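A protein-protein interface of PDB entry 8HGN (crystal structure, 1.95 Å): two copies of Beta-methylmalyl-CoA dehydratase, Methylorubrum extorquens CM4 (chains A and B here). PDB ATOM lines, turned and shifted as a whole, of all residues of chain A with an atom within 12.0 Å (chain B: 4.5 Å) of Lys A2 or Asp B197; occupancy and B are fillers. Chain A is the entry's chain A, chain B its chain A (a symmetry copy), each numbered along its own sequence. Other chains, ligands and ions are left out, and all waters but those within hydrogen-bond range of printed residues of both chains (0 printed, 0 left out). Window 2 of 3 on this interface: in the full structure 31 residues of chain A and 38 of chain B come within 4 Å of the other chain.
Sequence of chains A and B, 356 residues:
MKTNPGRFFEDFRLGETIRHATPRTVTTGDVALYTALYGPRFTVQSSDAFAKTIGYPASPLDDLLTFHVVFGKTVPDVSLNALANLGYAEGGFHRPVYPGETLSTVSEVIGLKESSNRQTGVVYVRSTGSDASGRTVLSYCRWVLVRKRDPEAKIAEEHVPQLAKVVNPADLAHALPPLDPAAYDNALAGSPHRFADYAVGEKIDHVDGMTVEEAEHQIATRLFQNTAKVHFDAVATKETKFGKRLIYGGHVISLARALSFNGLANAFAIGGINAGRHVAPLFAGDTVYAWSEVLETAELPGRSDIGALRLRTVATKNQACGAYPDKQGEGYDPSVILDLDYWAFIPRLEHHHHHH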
ATOM      1  N   LYS A   2      11.753 -11.004  -0.369  1.00  0.00           N
ATOM      2  CA  LYS A   2      10.992 -11.305  -1.620  1.00  0.00           C
ATOM      3  C   LYS A   2      11.218 -12.767  -2.062  1.00  0.00           C
ATOM      4  O   LYS A   2      10.488 -13.209  -2.995  1.00  0.00           O
ATOM      5  CB  LYS A   2      11.367 -10.290  -2.706  1.00  0.00           C
ATOM      6  CG  LYS A   2      10.957  -8.852  -2.420  1.00  0.00           C
ATOM      7  CD  LYS A   2      11.319  -7.878  -3.525  1.00  0.00           C
ATOM      8  CE  LYS A   2      10.695  -6.498  -3.378  1.00  0.00           C
ATOM      9  NZ  LYS A   2      11.646  -5.472  -2.890  1.00  0.00           N
ATOM     10  N   THR A   3      12.177 -13.478  -1.438  1.00  0.00           N
ATOM     11  CA  THR A   3      12.328 -14.966  -1.457  1.00  0.00           C
ATOM     12  C   THR A   3      10.986 -15.605  -1.090  1.00  0.00           C
ATOM     13  O   THR A   3      10.622 -15.547   0.103  1.00  0.00           O
ATOM     14  CB  THR A   3      13.371 -15.482  -0.450  1.00  0.00           C
ATOM     15  OG1 THR A   3      14.671 -15.003  -0.793  1.00  0.00           O
ATOM     16  CG2 THR A   3      13.421 -16.994  -0.368  1.00  0.00           C
ATOM     17  N   ASN A   4      10.301 -16.203  -2.071  1.00  0.00           N
ATOM     18  CA  ASN A   4       8.909 -16.706  -1.941  1.00  0.00           C
ATOM     19  C   ASN A   4       8.888 -18.153  -2.402  1.00  0.00           C
ATOM     20  O   ASN A   4       8.836 -18.400  -3.606  1.00  0.00           O
ATOM     21  CB  ASN A   4       7.921 -15.857  -2.754  1.00  0.00           C
ATOM     22  CG  ASN A   4       6.483 -16.337  -2.673  1.00  0.00           C
ATOM     23  OD1 ASN A   4       5.828 -16.545  -3.689  1.00  0.00           O
ATOM     24  ND2 ASN A   4       5.973 -16.517  -1.467  1.00  0.00           N
ATOM     25  N   PRO A   5       8.919 -19.143  -1.474  1.00  0.00           N
ATOM     26  CA  PRO A   5       8.713 -20.543  -1.838  1.00  0.00           C
ATOM     27  C   PRO A   5       7.260 -20.830  -2.268  1.00  0.00           C
ATOM     28  O   PRO A   5       7.028 -21.986  -2.669  1.00  0.00           O
ATOM     29  CB  PRO A   5       9.073 -21.374  -0.588  1.00  0.00           C
ATOM     30  CG  PRO A   5       9.633 -20.362   0.418  1.00  0.00           C
ATOM     31  CD  PRO A   5       9.166 -18.989  -0.033  1.00  0.00           C
ATOM     32  N   GLY A   6       6.366 -19.821  -2.182  1.00  0.00           N
ATOM     33  CA  GLY A   6       4.970 -19.850  -2.678  1.00  0.00           C
ATOM     34  C   GLY A   6       3.968 -20.002  -1.540  1.00  0.00           C
ATOM     35  O   GLY A   6       4.357 -19.733  -0.379  1.00  0.00           O
ATOM     36  N   ARG A   7       2.717 -20.379  -1.857  1.00  0.00           N
ATOM     37  CA  ARG A   7       1.641 -20.733  -0.884  1.00  0.00           C
ATOM     38  C   ARG A   7       1.604 -22.225  -0.581  1.00  0.00           C
ATOM     39  O   ARG A   7       1.644 -23.039  -1.552  1.00  0.00           O
ATOM     40  CB  ARG A   7       0.236 -20.462  -1.415  1.00  0.00           C
ATOM     41  CG  ARG A   7      -0.139 -18.998  -1.389  1.00  0.00           C
ATOM     42  CD  ARG A   7      -1.631 -18.938  -1.264  1.00  0.00           C
ATOM     43  NE  ARG A   7      -2.113 -17.594  -1.474  1.00  0.00           N
ATOM     44  CZ  ARG A   7      -3.380 -17.274  -1.391  1.00  0.00           C
ATOM     45  NH1 ARG A   7      -4.262 -18.225  -1.132  1.00  0.00           N
ATOM     46  NH2 ARG A   7      -3.763 -16.023  -1.585  1.00  0.00           N
ATOM     47  N   PHE A   8       1.455 -22.542   0.707  1.00  0.00           N
ATOM     48  CA  PHE A   8       1.285 -23.912   1.254  1.00  0.00           C
ATOM     49  C   PHE A   8      -0.133 -24.063   1.833  1.00  0.00           C
ATOM     50  O   PHE A   8      -0.905 -23.081   1.885  1.00  0.00           O
ATOM     51  CB  PHE A   8       2.423 -24.197   2.235  1.00  0.00           C
ATOM     52  CG  PHE A   8       3.786 -24.089   1.592  1.00  0.00           C
ATOM     53  CD1 PHE A   8       4.511 -25.223   1.278  1.00  0.00           C
ATOM     54  CD2 PHE A   8       4.339 -22.853   1.278  1.00  0.00           C
ATOM     55  CE1 PHE A   8       5.770 -25.130   0.696  1.00  0.00           C
ATOM     56  CE2 PHE A   8       5.585 -22.763   0.668  1.00  0.00           C
ATOM     57  CZ  PHE A   8       6.301 -23.902   0.399  1.00  0.00           C
ATOM     58  N   PRO A  76       0.824 -20.794 -10.092  1.00  0.00           N
ATOM     59  CA  PRO A  76       1.690 -20.077  -9.146  1.00  0.00           C
ATOM     60  C   PRO A  76       1.102 -19.878  -7.731  1.00  0.00           C
ATOM     61  O   PRO A  76       1.822 -20.039  -6.751  1.00  0.00           O
ATOM     62  CB  PRO A  76       1.877 -18.731  -9.840  1.00  0.00           C
ATOM     63  CG  PRO A  76       1.843 -19.071 -11.321  1.00  0.00           C
ATOM     64  CD  PRO A  76       0.800 -20.165 -11.423  1.00  0.00           C
ATOM     65  N   LEU A  80       1.644 -24.438  -6.967  1.00  0.00           N
ATOM     66  CA  LEU A  80       3.114 -24.344  -7.162  1.00  0.00           C
ATOM     67  C   LEU A  80       3.772 -25.422  -6.314  1.00  0.00           C
ATOM     68  O   LEU A  80       4.765 -26.027  -6.790  1.00  0.00           O
ATOM     69  CB  LEU A  80       3.568 -22.952  -6.731  1.00  0.00           C
ATOM     70  CG  LEU A  80       5.070 -22.748  -6.617  1.00  0.00           C
ATOM     71  CD1 LEU A  80       5.771 -23.075  -7.932  1.00  0.00           C
ATOM     72  CD2 LEU A  80       5.359 -21.314  -6.194  1.00  0.00           C
ATOM     73  N   ASN A  81       3.202 -25.661  -5.128  1.00  0.00           N
ATOM     74  CA  ASN A  81       3.753 -26.587  -4.102  1.00  0.00           C
ATOM     75  C   ASN A  81       2.873 -27.828  -3.981  1.00  0.00           C
ATOM     76  O   ASN A  81       2.843 -28.434  -2.892  1.00  0.00           O
ATOM     77  CB  ASN A  81       3.911 -25.863  -2.766  1.00  0.00           C
ATOM     78  CG  ASN A  81       4.951 -24.772  -2.860  1.00  0.00           C
ATOM     79  OD1 ASN A  81       6.075 -25.026  -3.290  1.00  0.00           O
ATOM     80  ND2 ASN A  81       4.585 -23.560  -2.501  1.00  0.00           N
ATOM     81  N   ARG A 149       3.828 -26.103   4.678  1.00  0.00           N
ATOM     82  CA  ARG A 149       5.211 -25.582   4.913  1.00  0.00           C
ATOM     83  C   ARG A 149       5.749 -26.192   6.215  1.00  0.00           C
ATOM     84  O   ARG A 149       6.766 -26.899   6.171  1.00  0.00           O
ATOM     85  CB  ARG A 149       5.175 -24.055   4.974  1.00  0.00           C
ATOM     86  CG  ARG A 149       6.487 -23.400   5.379  1.00  0.00           C
ATOM     87  CD  ARG A 149       6.191 -21.995   5.884  1.00  0.00           C
ATOM     88  NE  ARG A 149       5.613 -21.142   4.844  1.00  0.00           N
ATOM     89  CZ  ARG A 149       4.338 -20.767   4.741  1.00  0.00           C
ATOM     90  NH1 ARG A 149       3.429 -21.144   5.624  1.00  0.00           N
ATOM     91  NH2 ARG A 149       3.972 -20.000   3.731  1.00  0.00           N
ATOM     92  N   LYS A 229       6.507 -27.311  -9.094  1.00  0.00           N
ATOM     93  CA  LYS A 229       7.956 -27.661  -8.982  1.00  0.00           C
ATOM     94  C   LYS A 229       8.164 -29.151  -9.286  1.00  0.00           C
ATOM     95  O   LYS A 229       9.171 -29.506  -9.932  1.00  0.00           O
ATOM     96  CB  LYS A 229       8.465 -27.322  -7.574  1.00  0.00           C
ATOM     97  CG  LYS A 229       8.553 -25.850  -7.221  1.00  0.00           C
ATOM     98  CD  LYS A 229       8.391 -25.607  -5.729  1.00  0.00           C
ATOM     99  CE  LYS A 229       9.242 -24.489  -5.196  1.00  0.00           C
ATOM    100  NZ  LYS A 229       8.494 -23.722  -4.180  1.00  0.00           N
ATOM    101  N   PRO B 192       3.318  -6.182  -6.588  1.00  0.00           N
ATOM    102  CA  PRO B 192       3.060  -4.774  -6.248  1.00  0.00           C
ATOM    103  C   PRO B 192       4.306  -3.858  -6.265  1.00  0.00           C
ATOM    104  O   PRO B 192       4.151  -2.642  -6.375  1.00  0.00           O
ATOM    105  CB  PRO B 192       2.489  -4.892  -4.827  1.00  0.00           C
ATOM    106  CG  PRO B 192       3.223  -6.093  -4.230  1.00  0.00           C
ATOM    107  CD  PRO B 192       3.382  -7.053  -5.395  1.00  0.00           C
ATOM    108  N   HIS B 193       5.507  -4.448  -6.206  1.00  0.00           N
ATOM    109  CA  HIS B 193       6.812  -3.737  -6.089  1.00  0.00           C
ATOM    110  C   HIS B 193       7.119  -2.922  -7.357  1.00  0.00           C
ATOM    111  O   HIS B 193       7.186  -3.514  -8.453  1.00  0.00           O
ATOM    112  CB  HIS B 193       7.885  -4.760  -5.734  1.00  0.00           C
ATOM    113  CG  HIS B 193       7.538  -5.563  -4.525  1.00  0.00           C
ATOM    114  ND1 HIS B 193       6.909  -5.007  -3.427  1.00  0.00           N
ATOM    115  CD2 HIS B 193       7.706  -6.877  -4.246  1.00  0.00           C
ATOM    116  CE1 HIS B 193       6.719  -5.943  -2.509  1.00  0.00           C
ATOM    117  NE2 HIS B 193       7.221  -7.103  -2.983  1.00  0.00           N
ATOM    118  N   ARG B 194       7.262  -1.600  -7.209  1.00  0.00           N
ATOM    119  CA  ARG B 194       7.566  -0.623  -8.292  1.00  0.00           C
ATOM    120  C   ARG B 194       9.025  -0.175  -8.136  1.00  0.00           C
ATOM    121  O   ARG B 194       9.718  -0.713  -7.223  1.00  0.00           O
ATOM    122  CB  ARG B 194       6.583   0.557  -8.233  1.00  0.00           C
ATOM    123  CG  ARG B 194       5.119   0.181  -8.456  1.00  0.00           C
ATOM    124  CD  ARG B 194       4.818  -0.107  -9.908  1.00  0.00           C
ATOM    125  NE  ARG B 194       3.416  -0.295 -10.312  1.00  0.00           N
ATOM    126  CZ  ARG B 194       2.740   0.499 -11.168  1.00  0.00           C
ATOM    127  NH1 ARG B 194       3.291   1.591 -11.678  1.00  0.00           N
ATOM    128  NH2 ARG B 194       1.496   0.211 -11.516  1.00  0.00           N
ATOM    129  N   PHE B 195       9.494   0.737  -9.003  1.00  0.00           N
ATOM    130  CA  PHE B 195      10.878   1.289  -8.964  1.00  0.00           C
ATOM    131  C   PHE B 195      11.271   1.552  -7.504  1.00  0.00           C
ATOM    132  O   PHE B 195      12.312   1.057  -7.078  1.00  0.00           O
ATOM    133  CB  PHE B 195      10.976   2.542  -9.846  1.00  0.00           C
ATOM    134  CG  PHE B 195      12.318   3.240  -9.846  1.00  0.00           C
ATOM    135  CD1 PHE B 195      12.440   4.547  -9.394  1.00  0.00           C
ATOM    136  CD2 PHE B 195      13.455   2.601 -10.320  1.00  0.00           C
ATOM    137  CE1 PHE B 195      13.669   5.189  -9.401  1.00  0.00           C
ATOM    138  CE2 PHE B 195      14.685   3.242 -10.326  1.00  0.00           C
ATOM    139  CZ  PHE B 195      14.788   4.538  -9.870  1.00  0.00           C
ATOM    140  N   ALA B 196      10.411   2.263  -6.758  1.00  0.00           N
ATOM    141  CA  ALA B 196      10.695   2.832  -5.418  1.00  0.00           C
ATOM    142  C   ALA B 196      10.687   1.747  -4.339  1.00  0.00           C
ATOM    143  O   ALA B 196      11.069   2.056  -3.201  1.00  0.00           O
ATOM    144  CB  ALA B 196       9.713   3.946  -5.088  1.00  0.00           C
ATOM    145  N   ASP B 197      10.287   0.515  -4.654  1.00  0.00           N
ATOM    146  CA  ASP B 197      10.146  -0.546  -3.617  1.00  0.00           C
ATOM    147  C   ASP B 197      11.433  -1.367  -3.527  1.00  0.00           C
ATOM    148  O   ASP B 197      11.534  -2.238  -2.639  1.00  0.00           O
ATOM    149  CB  ASP B 197       8.901  -1.392  -3.875  1.00  0.00           C
ATOM    150  CG  ASP B 197       7.634  -0.634  -3.521  1.00  0.00           C
ATOM    151  OD1 ASP B 197       7.396  -0.447  -2.307  1.00  0.00           O
ATOM    152  OD2 ASP B 197       6.942  -0.179  -4.456  1.00  0.00           O
ATOM    153  N   TYR B 198      12.402  -1.083  -4.393  1.00  0.00           N
ATOM    154  CA  TYR B 198      13.683  -1.826  -4.394  1.00  0.00           C
ATOM    155  C   TYR B 198      14.718  -0.986  -3.645  1.00  0.00           C
ATOM    156  O   TYR B 198      14.750   0.236  -3.821  1.00  0.00           O
ATOM    157  CB  TYR B 198      14.037  -2.239  -5.825  1.00  0.00           C
ATOM    158  CG  TYR B 198      13.196  -3.400  -6.307  1.00  0.00           C
ATOM    159  CD1 TYR B 198      13.420  -4.678  -5.820  1.00  0.00           C
ATOM    160  CD2 TYR B 198      12.135  -3.208  -7.178  1.00  0.00           C
ATOM    161  CE1 TYR B 198      12.634  -5.746  -6.214  1.00  0.00           C
ATOM    162  CE2 TYR B 198      11.344  -4.263  -7.598  1.00  0.00           C
ATOM    163  CZ  TYR B 198      11.599  -5.531  -7.108  1.00  0.00           C
ATOM    164  OH  TYR B 198      10.850  -6.592  -7.510  1.00  0.00           O
ATOM    165  N   ALA B 199      15.490  -1.643  -2.781  1.00  0.00           N
ATOM    166  CA  ALA B 199      16.649  -1.052  -2.083  1.00  0.00           C
ATOM    167  C   ALA B 199      17.936  -1.657  -2.655  1.00  0.00           C
ATOM    168  O   ALA B 199      18.024  -2.906  -2.658  1.00  0.00           O
ATOM    169  CB  ALA B 199      16.549  -1.322  -0.605  1.00  0.00           C
ATOM    170  N   GLU B 202      19.580  -5.198  -1.606  1.00  0.00           N
ATOM    171  CA  GLU B 202      18.562  -6.275  -1.461  1.00  0.00           C
ATOM    172  C   GLU B 202      19.003  -7.544  -2.217  1.00  0.00           C
ATOM    173  O   GLU B 202      19.502  -7.410  -3.356  1.00  0.00           O
ATOM    174  CB  GLU B 202      17.211  -5.788  -1.973  1.00  0.00           C
ATOM    175  CG  GLU B 202      16.159  -6.874  -1.987  1.00  0.00           C
ATOM    176  CD  GLU B 202      14.765  -6.329  -2.172  1.00  0.00           C
ATOM    177  OE1 GLU B 202      13.839  -7.126  -1.996  1.00  0.00           O
ATOM    178  OE2 GLU B 202      14.626  -5.106  -2.459  1.00  0.00           O
ATOM    179  N   ILE B 204      17.713 -11.654  -3.318  1.00  0.00           N
ATOM    180  CA  ILE B 204      16.455 -12.378  -3.674  1.00  0.00           C
ATOM    181  C   ILE B 204      16.834 -13.784  -4.145  1.00  0.00           C
ATOM    182  O   ILE B 204      17.405 -13.927  -5.225  1.00  0.00           O
ATOM    183  CB  ILE B 204      15.663 -11.581  -4.731  1.00  0.00           C
ATOM    184  CG1 ILE B 204      15.365 -10.156  -4.264  1.00  0.00           C
ATOM    185  CG2 ILE B 204      14.392 -12.308  -5.163  1.00  0.00           C
ATOM    186  CD1 ILE B 204      14.632  -9.326  -5.286  1.00  0.00           C
ATOM    187  N   GLY B 263      10.349 -12.558  -7.791  1.00  0.00           N
ATOM    188  CA  GLY B 263      10.942 -11.431  -7.025  1.00  0.00           C
ATOM    189  C   GLY B 263      11.164 -10.154  -7.839  1.00  0.00           C
ATOM    190  O   GLY B 263      11.229  -9.060  -7.192  1.00  0.00           O
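NZ of Lys A2 lies within hydrogen-bond range of O of Asp B197. NZ of Lys A2 is in salt-bridge range of OE1 of Glu B202, at 2.9 Å.
N of Arg B194 sits at hydrogen-bond distance from OD2 of Asp B197 (3.1 Å). The backbone carbonyl oxygen (O) of Gly B263 lies within hydrogen-bond range of the side-chain hydroxyl (OH) of Tyr B198 (2.5 Å).
Among the printed residues, pairs that only touch across the chains: Lys A2 with His B193 (3.1 Å), Lys A2 with Tyr B198 (3.5 Å) and Lys A2 with Gly B263 (3.9 Å).
Arg A7 touches none of the printed residues of chain B. Phe A8 touches none of the printed residues of chain B. No residue of chain A comes within 4 Å of Ala B196. Printed residues of chain A within 4 Å of Asp B197: Lys A2 (3.2 Å). No residue of chain A comes within 4 Å of Ala B199. Of the printed residues of chain A, Glu B202 touches Lys A2 (2.9 Å). No residue of chain A comes within 4 Å of Ile B204. Gly B263 touches just one residue of chain A: Lys A2 (3.9 Å). The nearest residue of chain B that does not touch Lys A2 is Ile B204 (4.02 Å). The nearest residue of chain A that does not touch Asp B197 is Thr A3 (11.3 Å). The nearest printed residue of chain A that does not touch Glu B202 is Thr A3 (6.6 Å).
Printed residues of chain B that touch a printed residue of chain A: His B193, Asp B197, Tyr B198, Glu B202 and Gly B263. Hydrophobic or aromatic side chains of chain B that line the printed part of chain A: His B193 and Tyr B198.
No position is printed for both chains. Of the 5 pairs that touch across the chains among the printed residues, none has its exchanged pair printed and touching as well.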
